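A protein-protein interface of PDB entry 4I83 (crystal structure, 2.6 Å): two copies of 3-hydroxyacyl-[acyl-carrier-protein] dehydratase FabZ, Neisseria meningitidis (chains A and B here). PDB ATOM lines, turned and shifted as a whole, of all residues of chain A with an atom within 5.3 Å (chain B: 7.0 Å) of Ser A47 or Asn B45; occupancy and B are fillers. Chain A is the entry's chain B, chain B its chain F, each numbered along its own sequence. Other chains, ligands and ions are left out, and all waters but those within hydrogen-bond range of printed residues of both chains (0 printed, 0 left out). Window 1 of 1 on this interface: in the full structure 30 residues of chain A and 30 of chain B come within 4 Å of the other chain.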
ATOM      1  N   ASN A  45      10.694  10.556  30.542  1.00  0.00           N
ATOM      2  CA  ASN A  45      10.828   9.150  30.284  1.00  0.00           C
ATOM      3  C   ASN A  45      12.297   8.734  30.366  1.00  0.00           C
ATOM      4  O   ASN A  45      13.141   9.361  29.783  1.00  0.00           O
ATOM      5  CB  ASN A  45      10.271   8.823  28.890  1.00  0.00           C
ATOM      6  CG  ASN A  45       8.768   8.600  28.891  1.00  0.00           C
ATOM      7  OD1 ASN A  45       8.171   8.371  29.918  1.00  0.00           O
ATOM      8  ND2 ASN A  45       8.161   8.666  27.728  1.00  0.00           N
ATOM      9  N   VAL A  46      12.589   7.654  31.073  1.00  0.00           N
ATOM     10  CA  VAL A  46      13.953   7.154  31.145  1.00  0.00           C
ATOM     11  C   VAL A  46      14.114   5.961  30.205  1.00  0.00           C
ATOM     12  O   VAL A  46      13.394   4.960  30.330  1.00  0.00           O
ATOM     13  CB  VAL A  46      14.351   6.759  32.588  1.00  0.00           C
ATOM     14  CG1 VAL A  46      15.784   6.269  32.636  1.00  0.00           C
ATOM     15  CG2 VAL A  46      14.168   7.957  33.493  1.00  0.00           C
ATOM     16  N   SER A  47      15.060   6.087  29.287  1.00  0.00           N
ATOM     17  CA  SER A  47      15.272   5.103  28.259  1.00  0.00           C
ATOM     18  C   SER A  47      16.749   4.744  28.206  1.00  0.00           C
ATOM     19  O   SER A  47      17.604   5.573  28.511  1.00  0.00           O
ATOM     20  CB  SER A  47      14.843   5.660  26.912  1.00  0.00           C
ATOM     21  OG  SER A  47      15.132   4.749  25.883  1.00  0.00           O
ATOM     22  N   ILE A  48      17.032   3.504  27.831  1.00  0.00           N
ATOM     23  CA  ILE A  48      18.408   3.029  27.681  1.00  0.00           C
ATOM     24  C   ILE A  48      19.063   3.773  26.518  1.00  0.00           C
ATOM     25  O   ILE A  48      20.292   3.896  26.475  1.00  0.00           O
ATOM     26  CB  ILE A  48      18.463   1.491  27.509  1.00  0.00           C
ATOM     27  CG1 ILE A  48      19.869   0.952  27.533  1.00  0.00           C
ATOM     28  CG2 ILE A  48      17.861   1.072  26.178  1.00  0.00           C
ATOM     29  CD1 ILE A  48      20.625   1.211  28.800  1.00  0.00           C
ATOM     30  N   ASN A  49      18.262   4.315  25.609  1.00  0.00           N
ATOM     31  CA  ASN A  49      18.793   5.107  24.489  1.00  0.00           C
ATOM     32  C   ASN A  49      19.074   6.578  24.835  1.00  0.00           C
ATOM     33  O   ASN A  49      18.812   7.455  24.046  1.00  0.00           O
ATOM     34  CB  ASN A  49      17.810   5.043  23.313  1.00  0.00           C
ATOM     35  CG  ASN A  49      18.421   5.472  22.010  1.00  0.00           C
ATOM     36  OD1 ASN A  49      19.566   5.145  21.700  1.00  0.00           O
ATOM     37  ND2 ASN A  49      17.673   6.257  21.251  1.00  0.00           N
ATOM     38  N   GLU A  50      19.619   6.837  26.012  1.00  0.00           N
ATOM     39  CA  GLU A  50      19.992   8.199  26.411  1.00  0.00           C
ATOM     40  C   GLU A  50      21.520   8.312  26.600  1.00  0.00           C
ATOM     41  O   GLU A  50      22.147   7.354  27.023  1.00  0.00           O
ATOM     42  CB  GLU A  50      19.290   8.571  27.689  1.00  0.00           C
ATOM     43  CG  GLU A  50      17.804   8.776  27.534  1.00  0.00           C
ATOM     44  CD  GLU A  50      17.178   9.327  28.791  1.00  0.00           C
ATOM     45  OE1 GLU A  50      16.340   8.614  29.379  1.00  0.00           O
ATOM     46  OE2 GLU A  50      17.541  10.438  29.226  1.00  0.00           O
ATOM     47  N   PHE A  53      23.772   6.913  29.550  1.00  0.00           N
ATOM     48  CA  PHE A  53      23.910   5.483  29.818  1.00  0.00           C
ATOM     49  C   PHE A  53      25.073   4.805  29.111  1.00  0.00           C
ATOM     50  O   PHE A  53      25.299   3.654  29.362  1.00  0.00           O
ATOM     51  CB  PHE A  53      22.600   4.760  29.551  1.00  0.00           C
ATOM     52  CG  PHE A  53      21.498   5.190  30.460  1.00  0.00           C
ATOM     53  CD1 PHE A  53      21.620   5.030  31.835  1.00  0.00           C
ATOM     54  CD2 PHE A  53      20.359   5.787  29.961  1.00  0.00           C
ATOM     55  CE1 PHE A  53      20.605   5.442  32.683  1.00  0.00           C
ATOM     56  CE2 PHE A  53      19.341   6.200  30.796  1.00  0.00           C
ATOM     57  CZ  PHE A  53      19.465   6.024  32.159  1.00  0.00           C
ATOM     58  N   PRO A 109      16.100   2.402  33.081  1.00  0.00           N
ATOM     59  CA  PRO A 109      15.383   2.434  31.807  1.00  0.00           C
ATOM     60  C   PRO A 109      14.026   1.708  31.879  1.00  0.00           C
ATOM     61  O   PRO A 109      13.933   0.616  32.476  1.00  0.00           O
ATOM     62  CB  PRO A 109      16.303   1.691  30.855  1.00  0.00           C
ATOM     63  CG  PRO A 109      17.661   1.822  31.453  1.00  0.00           C
ATOM     64  CD  PRO A 109      17.513   2.030  32.919  1.00  0.00           C
ATOM     65  N   GLY A 110      12.988   2.335  31.316  1.00  0.00           N
ATOM     66  CA  GLY A 110      11.639   1.836  31.468  1.00  0.00           C
ATOM     67  C   GLY A 110      10.837   2.675  32.437  1.00  0.00           C
ATOM     68  O   GLY A 110       9.634   2.821  32.248  1.00  0.00           O
ATOM     69  N   ASP A 111      11.481   3.259  33.453  1.00  0.00           N
ATOM     70  CA  ASP A 111      10.779   4.123  34.393  1.00  0.00           C
ATOM     71  C   ASP A 111      10.364   5.420  33.776  1.00  0.00           C
ATOM     72  O   ASP A 111      11.141   6.050  33.060  1.00  0.00           O
ATOM     73  CB  ASP A 111      11.637   4.469  35.621  1.00  0.00           C
ATOM     74  CG  ASP A 111      11.922   3.281  36.492  1.00  0.00           C
ATOM     75  OD1 ASP A 111      11.269   2.231  36.332  1.00  0.00           O
ATOM     76  OD2 ASP A 111      12.826   3.379  37.337  1.00  0.00           O
ATOM     77  N   GLN A 112       9.154   5.838  34.107  1.00  0.00           N
ATOM     78  CA  GLN A 112       8.682   7.158  33.793  1.00  0.00           C
ATOM     79  C   GLN A 112       8.717   8.033  35.048  1.00  0.00           C
ATOM     80  O   GLN A 112       8.120   7.696  36.051  1.00  0.00           O
ATOM     81  CB  GLN A 112       7.287   7.071  33.238  1.00  0.00           C
ATOM     82  CG  GLN A 112       6.654   8.430  33.058  1.00  0.00           C
ATOM     83  CD  GLN A 112       5.405   8.358  32.193  1.00  0.00           C
ATOM     84  OE1 GLN A 112       5.477   8.081  30.979  1.00  0.00           O
ATOM     85  NE2 GLN A 112       4.242   8.657  32.809  1.00  0.00           N
ATOM     86  N   ALA B  12      16.498  -3.674  31.199  1.00  0.00           N
ATOM     87  CA  ALA B  12      17.473  -3.367  30.161  1.00  0.00           C
ATOM     88  C   ALA B  12      18.824  -4.022  30.420  1.00  0.00           C
ATOM     89  O   ALA B  12      19.395  -4.643  29.530  1.00  0.00           O
ATOM     90  CB  ALA B  12      17.650  -1.857  30.030  1.00  0.00           C
ATOM     91  N   LEU B  26      20.011  -0.082  20.838  1.00  0.00           N
ATOM     92  CA  LEU B  26      19.181  -0.904  21.689  1.00  0.00           C
ATOM     93  C   LEU B  26      17.887  -0.139  21.888  1.00  0.00           C
ATOM     94  O   LEU B  26      17.898   0.928  22.522  1.00  0.00           O
ATOM     95  CB  LEU B  26      19.866  -1.162  23.009  1.00  0.00           C
ATOM     96  CG  LEU B  26      19.088  -1.989  24.037  1.00  0.00           C
ATOM     97  CD1 LEU B  26      18.480  -3.226  23.410  1.00  0.00           C
ATOM     98  CD2 LEU B  26      20.026  -2.356  25.193  1.00  0.00           C
ATOM     99  N   GLN B  27      16.780  -0.672  21.350  1.00  0.00           N
ATOM    100  CA  GLN B  27      15.509   0.057  21.296  1.00  0.00           C
ATOM    101  C   GLN B  27      14.426  -0.612  22.100  1.00  0.00           C
ATOM    102  O   GLN B  27      13.225  -0.411  21.844  1.00  0.00           O
ATOM    103  CB  GLN B  27      15.032   0.213  19.858  1.00  0.00           C
ATOM    104  CG  GLN B  27      15.901   1.110  18.981  1.00  0.00           C
ATOM    105  CD  GLN B  27      16.004   2.538  19.480  1.00  0.00           C
ATOM    106  OE1 GLN B  27      17.104   3.080  19.631  1.00  0.00           O
ATOM    107  NE2 GLN B  27      14.875   3.161  19.731  1.00  0.00           N
ATOM    108  N   LEU B  28      14.832  -1.390  23.100  1.00  0.00           N
ATOM    109  CA  LEU B  28      13.903  -1.902  24.112  1.00  0.00           C
ATOM    110  C   LEU B  28      14.421  -1.503  25.486  1.00  0.00           C
ATOM    111  O   LEU B  28      15.614  -1.617  25.758  1.00  0.00           O
ATOM    112  CB  LEU B  28      13.812  -3.426  24.042  1.00  0.00           C
ATOM    113  CG  LEU B  28      13.296  -4.054  22.748  1.00  0.00           C
ATOM    114  CD1 LEU B  28      13.339  -5.570  22.856  1.00  0.00           C
ATOM    115  CD2 LEU B  28      11.894  -3.554  22.444  1.00  0.00           C
ATOM    116  N   ASP B  29      13.518  -1.044  26.343  1.00  0.00           N
ATOM    117  CA  ASP B  29      13.874  -0.707  27.709  1.00  0.00           C
ATOM    118  C   ASP B  29      13.579  -1.825  28.711  1.00  0.00           C
ATOM    119  O   ASP B  29      14.308  -1.985  29.686  1.00  0.00           O
ATOM    120  CB  ASP B  29      13.178   0.593  28.110  1.00  0.00           C
ATOM    121  CG  ASP B  29      13.717   1.796  27.339  1.00  0.00           C
ATOM    122  OD1 ASP B  29      14.893   1.758  26.893  1.00  0.00           O
ATOM    123  OD2 ASP B  29      12.980   2.786  27.183  1.00  0.00           O
ATOM    124  N   ARG B  30      12.531  -2.608  28.463  1.00  0.00           N
ATOM    125  CA  ARG B  30      12.065  -3.586  29.450  1.00  0.00           C
ATOM    126  C   ARG B  30      11.119  -4.613  28.815  1.00  0.00           C
ATOM    127  O   ARG B  30      10.247  -4.239  28.041  1.00  0.00           O
ATOM    128  CB  ARG B  30      11.324  -2.854  30.551  1.00  0.00           C
ATOM    129  CG  ARG B  30      10.935  -3.715  31.753  1.00  0.00           C
ATOM    130  CD  ARG B  30      10.257  -2.851  32.823  1.00  0.00           C
ATOM    131  NE  ARG B  30      11.207  -1.917  33.463  1.00  0.00           N
ATOM    132  CZ  ARG B  30      10.863  -0.792  34.090  1.00  0.00           C
ATOM    133  NH1 ARG B  30       9.601  -0.429  34.198  1.00  0.00           N
ATOM    134  NH2 ARG B  30      11.787  -0.012  34.601  1.00  0.00           N
ATOM    135  N   ILE B  43       8.510  -2.722  26.442  1.00  0.00           N
ATOM    136  CA  ILE B  43       8.346  -1.275  26.311  1.00  0.00           C
ATOM    137  C   ILE B  43       9.630  -0.536  25.912  1.00  0.00           C
ATOM    138  O   ILE B  43      10.749  -1.021  26.080  1.00  0.00           O
ATOM    139  CB  ILE B  43       7.757  -0.636  27.586  1.00  0.00           C
ATOM    140  CG1 ILE B  43       8.683  -0.812  28.787  1.00  0.00           C
ATOM    141  CG2 ILE B  43       6.395  -1.235  27.897  1.00  0.00           C
ATOM    142  CD1 ILE B  43       8.267   0.030  29.975  1.00  0.00           C
ATOM    143  N   LYS B  44       9.423   0.642  25.360  1.00  0.00           N
ATOM    144  CA  LYS B  44      10.497   1.573  25.026  1.00  0.00           C
ATOM    145  C   LYS B  44       9.979   2.947  25.346  1.00  0.00           C
ATOM    146  O   LYS B  44       8.967   3.372  24.788  1.00  0.00           O
ATOM    147  CB  LYS B  44      10.855   1.479  23.542  1.00  0.00           C
ATOM    148  CG  LYS B  44      12.108   2.233  23.130  1.00  0.00           C
ATOM    149  CD  LYS B  44      11.832   3.693  22.817  1.00  0.00           C
ATOM    150  CE  LYS B  44      13.083   4.380  22.271  1.00  0.00           C
ATOM    151  NZ  LYS B  44      14.088   4.692  23.320  1.00  0.00           N
ATOM    152  N   ASN B  45      10.628   3.612  26.287  1.00  0.00           N
ATOM    153  CA  ASN B  45      10.274   4.977  26.645  1.00  0.00           C
ATOM    154  C   ASN B  45      10.847   5.985  25.637  1.00  0.00           C
ATOM    155  O   ASN B  45      12.006   5.872  25.248  1.00  0.00           O
ATOM    156  CB  ASN B  45      10.838   5.293  28.015  1.00  0.00           C
ATOM    157  CG  ASN B  45       9.917   4.875  29.132  1.00  0.00           C
ATOM    158  OD1 ASN B  45       8.750   4.595  28.915  1.00  0.00           O
ATOM    159  ND2 ASN B  45      10.440   4.835  30.336  1.00  0.00           N
ATOM    160  N   VAL B  46      10.036   6.932  25.183  1.00  0.00           N
ATOM    161  CA  VAL B  46      10.511   7.902  24.223  1.00  0.00           C
ATOM    162  C   VAL B  46      10.757   9.201  24.954  1.00  0.00           C
ATOM    163  O   VAL B  46       9.856   9.749  25.568  1.00  0.00           O
ATOM    164  CB  VAL B  46       9.531   8.105  23.045  1.00  0.00           C
ATOM    165  CG1 VAL B  46      10.085   9.123  22.062  1.00  0.00           C
ATOM    166  CG2 VAL B  46       9.299   6.798  22.328  1.00  0.00           C
ATOM    167  N   SER B  47      11.994   9.678  24.859  1.00  0.00           N
ATOM    168  CA  SER B  47      12.429  10.861  25.556  1.00  0.00           C
ATOM    169  C   SER B  47      13.096  11.821  24.583  1.00  0.00           C
ATOM    170  O   SER B  47      13.721  11.392  23.619  1.00  0.00           O
ATOM    171  CB  SER B  47      13.422  10.474  26.641  1.00  0.00           C
ATOM    172  OG  SER B  47      13.928  11.628  27.298  1.00  0.00           O
ATOM    173  N   ASN B  49      15.636  13.361  25.295  1.00  0.00           N
ATOM    174  CA  ASN B  49      17.071  13.153  25.510  1.00  0.00           C
ATOM    175  C   ASN B  49      17.615  11.923  24.817  1.00  0.00           C
ATOM    176  O   ASN B  49      18.405  11.174  25.387  1.00  0.00           O
ATOM    177  CB  ASN B  49      17.361  13.061  27.024  1.00  0.00           C
ATOM    178  CG  ASN B  49      18.832  13.214  27.367  1.00  0.00           C
ATOM    179  OD1 ASN B  49      19.553  13.993  26.768  1.00  0.00           O
ATOM    180  ND2 ASN B  49      19.285  12.417  28.309  1.00  0.00           N
ATOM    181  N   GLU B  50      17.199  11.699  23.581  1.00  0.00           N
ATOM    182  CA  GLU B  50      17.705  10.560  22.804  1.00  0.00           C
ATOM    183  C   GLU B  50      18.451  11.070  21.564  1.00  0.00           C
ATOM    184  O   GLU B  50      18.053  12.082  20.989  1.00  0.00           O
ATOM    185  CB  GLU B  50      16.548   9.667  22.388  1.00  0.00           C
ATOM    186  CG  GLU B  50      15.930   8.870  23.512  1.00  0.00           C
ATOM    187  CD  GLU B  50      14.910   7.867  23.007  1.00  0.00           C
ATOM    188  OE1 GLU B  50      13.730   7.996  23.367  1.00  0.00           O
ATOM    189  OE2 GLU B  50      15.286   6.939  22.258  1.00  0.00           O
ATOM    190  N   GLN B  52      18.634  10.498  18.419  1.00  0.00           N
ATOM    191  CA  GLN B  52      17.947  10.719  17.145  1.00  0.00           C
ATOM    192  C   GLN B  52      17.270  12.084  17.072  1.00  0.00           C
ATOM    193  O   GLN B  52      17.069  12.631  15.987  1.00  0.00           O
ATOM    194  CB  GLN B  52      16.931   9.612  16.840  1.00  0.00           C
ATOM    195  CG  GLN B  52      15.780   9.481  17.830  1.00  0.00           C
ATOM    196  CD  GLN B  52      16.091   8.561  19.007  1.00  0.00           C
ATOM    197  OE1 GLN B  52      17.244   8.340  19.350  1.00  0.00           O
ATOM    198  NE2 GLN B  52      15.051   8.035  19.620  1.00  0.00           N
ATOM    199  N   MET B  63       9.650  10.596  16.768  1.00  0.00           N
ATOM    200  CA  MET B  63      10.304   9.313  16.824  1.00  0.00           C
ATOM    201  C   MET B  63      10.294   8.683  15.426  1.00  0.00           C
ATOM    202  O   MET B  63       9.244   8.488  14.848  1.00  0.00           O
ATOM    203  CB  MET B  63       9.574   8.416  17.803  1.00  0.00           C
ATOM    204  CG  MET B  63      10.127   7.000  17.882  1.00  0.00           C
ATOM    205  SD  MET B  63      11.705   6.949  18.698  1.00  0.00           S
ATOM    206  CE  MET B  63      12.029   5.190  18.740  1.00  0.00           C
ATOM    207  N   ILE B 108       5.951  10.712  20.076  1.00  0.00           N
ATOM    208  CA  ILE B 108       6.691  11.909  20.527  1.00  0.00           C
ATOM    209  C   ILE B 108       7.267  11.753  21.929  1.00  0.00           C
ATOM    210  O   ILE B 108       6.852  10.862  22.675  1.00  0.00           O
ATOM    211  CB  ILE B 108       5.799  13.203  20.437  1.00  0.00           C
ATOM    212  CG1 ILE B 108       4.505  13.061  21.242  1.00  0.00           C
ATOM    213  CG2 ILE B 108       5.456  13.521  18.977  1.00  0.00           C
ATOM    214  CD1 ILE B 108       3.761  14.373  21.402  1.00  0.00           C
ATOM    215  N   GLY B 110       7.788  11.674  25.684  1.00  0.00           N
ATOM    216  CA  GLY B 110       6.727  11.513  26.672  1.00  0.00           C
ATOM    217  C   GLY B 110       5.914  10.242  26.439  1.00  0.00           C
ATOM    218  O   GLY B 110       5.450   9.656  27.379  1.00  0.00           O
ATOM    219  N   ASP B 111       5.790   9.799  25.189  1.00  0.00           N
ATOM    220  CA  ASP B 111       5.109   8.526  24.893  1.00  0.00           C
ATOM    221  C   ASP B 111       5.900   7.325  25.349  1.00  0.00           C
ATOM    222  O   ASP B 111       7.113   7.269  25.162  1.00  0.00           O
ATOM    223  CB  ASP B 111       4.845   8.338  23.396  1.00  0.00           C
ATOM    224  CG  ASP B 111       3.877   9.351  22.841  1.00  0.00           C
ATOM    225  OD1 ASP B 111       3.192  10.025  23.626  1.00  0.00           O
ATOM    226  OD2 ASP B 111       3.820   9.467  21.607  1.00  0.00           O
ATOM    227  N   GLN B 112       5.185   6.364  25.917  1.00  0.00           N
ATOM    228  CA  GLN B 112       5.734   5.070  26.206  1.00  0.00           C
ATOM    229  C   GLN B 112       5.213   4.106  25.143  1.00  0.00           C
ATOM    230  O   GLN B 112       4.012   3.921  24.987  1.00  0.00           O
ATOM    231  CB  GLN B 112       5.340   4.633  27.602  1.00  0.00           C
ATOM    232  CG  GLN B 112       5.714   3.197  27.883  1.00  0.00           C
ATOM    233  CD  GLN B 112       5.649   2.827  29.350  1.00  0.00           C
ATOM    234  OE1 GLN B 112       6.451   3.307  30.162  1.00  0.00           O
ATOM    235  NE2 GLN B 112       4.677   1.961  29.704  1.00  0.00           N
ATOM    236  N   LEU B 113       6.125   3.505  24.383  1.00  0.00           N
ATOM    237  CA  LEU B 113       5.729   2.562  23.376  1.00  0.00           C
ATOM    238  C   LEU B 113       5.552   1.220  24.053  1.00  0.00           C
ATOM    239  O   LEU B 113       6.479   0.736  24.714  1.00  0.00           O
ATOM    240  CB  LEU B 113       6.771   2.472  22.247  1.00  0.00           C
ATOM    241  CG  LEU B 113       6.704   3.611  21.224  1.00  0.00           C
ATOM    242  CD1 LEU B 113       8.015   3.748  20.455  1.00  0.00           C
ATOM    243  CD2 LEU B 113       5.546   3.415  20.248  1.00  0.00           C
ATOM    244  N   PHE B 115       5.087  -2.664  22.978  1.00  0.00           N
ATOM    245  CA  PHE B 115       5.238  -3.586  21.838  1.00  0.00           C
ATOM    246  C   PHE B 115       4.652  -4.934  22.204  1.00  0.00           C
ATOM    247  O   PHE B 115       5.053  -5.508  23.199  1.00  0.00           O
ATOM    248  CB  PHE B 115       6.717  -3.780  21.466  1.00  0.00           C
ATOM    249  CG  PHE B 115       7.413  -2.521  21.072  1.00  0.00           C
ATOM    250  CD1 PHE B 115       7.243  -1.971  19.813  1.00  0.00           C
ATOM    251  CD2 PHE B 115       8.257  -1.876  21.973  1.00  0.00           C
ATOM    252  CE1 PHE B 115       7.893  -0.787  19.460  1.00  0.00           C
ATOM    253  CE2 PHE B 115       8.900  -0.692  21.629  1.00  0.00           C
ATOM    254  CZ  PHE B 115       8.722  -0.144  20.370  1.00  0.00           C
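The backbone NH (N) of Ile B108 is in hydrogen-bond range of the side-chain carboxylate (OD2) of Asp B111, at 2.9 Å. The backbone NH of Ala B12 is in hydrogen-bond range of the backbone carbonyl oxygen of Asp B29, 3.2 Å away. The backbone carbonyl oxygen (O) of Asp B111 is in hydrogen-bond range of the backbone NH (N) of Val B46, at 2.9 Å. OE2 of Glu B50 is in hydrogen-bond range of NE2 of Gln B52 (2.9 Å). N of Ser A47 sits at hydrogen-bond distance from OE1 of Glu A50, at 2.8 Å. OG of Ser A47 lies close to N of Asn A49 (3.2 Å).
Of the printed residues of chain B, Asn A45 touches Asn B45 (3.7 Å), Val B46 (3.0 Å), Ser B47 (3.3 Å), Gly B110 (2.9 Å) and Asp B111 (3.1 Å). Ser A47 touches just these residues of chain B: Asp B29, Lys B44 and Asn B45. Of the printed residues of chain B, Asn A49 touches Gln B27, Lys B44, Asn B49, Glu B50 and Gln B52. Phe A53 touches none of the printed residues of chain B. Of the printed residues of chain A, Leu B26 touches Ile A48 (3.7 Å). Asn B45 touches five residues of chain A. Met B63 touches none of the printed residues of chain A. The nearest residue of chain B that does not touch Ser A47 is Glu B50 (4.2 Å). The nearest residue of chain A that does not touch Asn B45 is Gln A112 (4.1 Å). The nearest printed residue of chain B that does not touch Asn A45 is Gln B112 (4.2 Å).
Asn B45 touches its own counterpart, Asn A45. Asn A45 touches Val B46, and with the chains exchanged Val A46 touches Asn B45. Asn A45 touches Gly B110, and with the chains exchanged Gly A110 touches Asn B45. Gly A110 touches Gln B112, and with the chains exchanged Gln A112 touches Gly B110. 8 positions are printed for both chains.
Asn A45 touches Asn B45 (CB to CB, 3.7 Å). CG2 of Ile A48 touches O of Leu B26, 3.7 Å away. ND2 of Asn A49 touches OE1 of Gln B27 (3.6 Å). Lys B44 touches Asn A49 (NZ to CB, 3.7 Å). Asn A49 touches Asn B49 (O to O, 3.97 Å). Pro A109 touches Ala B12. Pro A109 touches Asp B29 (O to O, 3.8 Å). Arg B30 touches Gly A110 (NH2 to C, 3.6 Å). Ile B43 touches Gly A110. O of Gly A110 touches OE1 of Gln B112 (3.8 Å).
The backbone carbonyl oxygen of Asp B111 lies within hydrogen-bond range of the side-chain amide nitrogen of Asn A45, at 3.1 Å. The side-chain carboxylate (OD1) of Asp B29 lies within hydrogen-bond range of the backbone NH (N) of Ile A48. NH2 of Arg B30 is in hydrogen-bond range of O of Pro A109 (3.1 Å). The backbone carbonyl oxygen of Asp A111 is in hydrogen-bond range of the side-chain amide nitrogen of Asn B45, at 3.1 Å. The side-chain carboxylate (OE2) of Glu B50 sits at hydrogen-bond distance from the side-chain amide nitrogen (ND2) of Asn A49 (2.7 Å). The side-chain hydroxyl (OG) of Ser A47 sits at hydrogen-bond distance from the side-chain carboxylate (OD1) of Asp B29 (3.2 Å). The side-chain hydroxyl (OG) of Ser A47 lies close to the backbone carbonyl oxygen (O) of Asn B45 (3.4 Å). The backbone carbonyl oxygen of Asn A45 sits close to the side-chain hydroxyl of Ser B47, 3.5 Å away. OE1 of Gln B52 is in hydrogen-bond range of ND2 of Asn A49 (2.9 Å). The backbone carbonyl oxygen of Val A46 is in hydrogen-bond range of the side-chain amide nitrogen of Asn B45 (3.0 Å). The side-chain carboxylate (OE2) of Glu A50 sits at hydrogen-bond distance from the side-chain amide nitrogen (ND2) of Asn B49 (2.8 Å). O of Gly A110 sits at hydrogen-bond distance from ND2 of Asn B45 (2.9 Å). The side-chain hydroxyl (OG) of Ser A47 sits at hydrogen-bond distance from the side-chain amino group (NZ) of Lys B44 (2.8 Å). O of Val B46 lies within hydrogen-bond range of ND2 of Asn A45 (3.0 Å). The backbone carbonyl oxygen of Gly B110 lies within hydrogen-bond range of the side-chain amide nitrogen of Asn A45 (2.9 Å). The guanidinium group of Arg B30 is in salt-bridge range of the side-chain carboxylate of Asp A111.
Hydrophobic or aromatic side chains of chain A within 4 Å of the printed part of chain B: Ile A48 and Pro A109. Of the 21 printed residues of chain B, 17 touch a printed residue of chain A. Printed residues of chain B that touch a printed residue of chain A: Ala B12, Leu B26, Gln B27, Leu B28, Asp B29, Arg B30, Ile B43, Lys B44, Asn B45, Val B46, Ser B47, Asn B49, Glu B50, Gln B52, Gly B110, Asp B111 and Gln B112. Hydrophobic or aromatic side chains of chain B within 4 Å of the printed part of chain A: Ala B12, Leu B26 and Ile B43. Along chain B the printed residues that touch a printed residue of chain A span positions 12 to 112.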
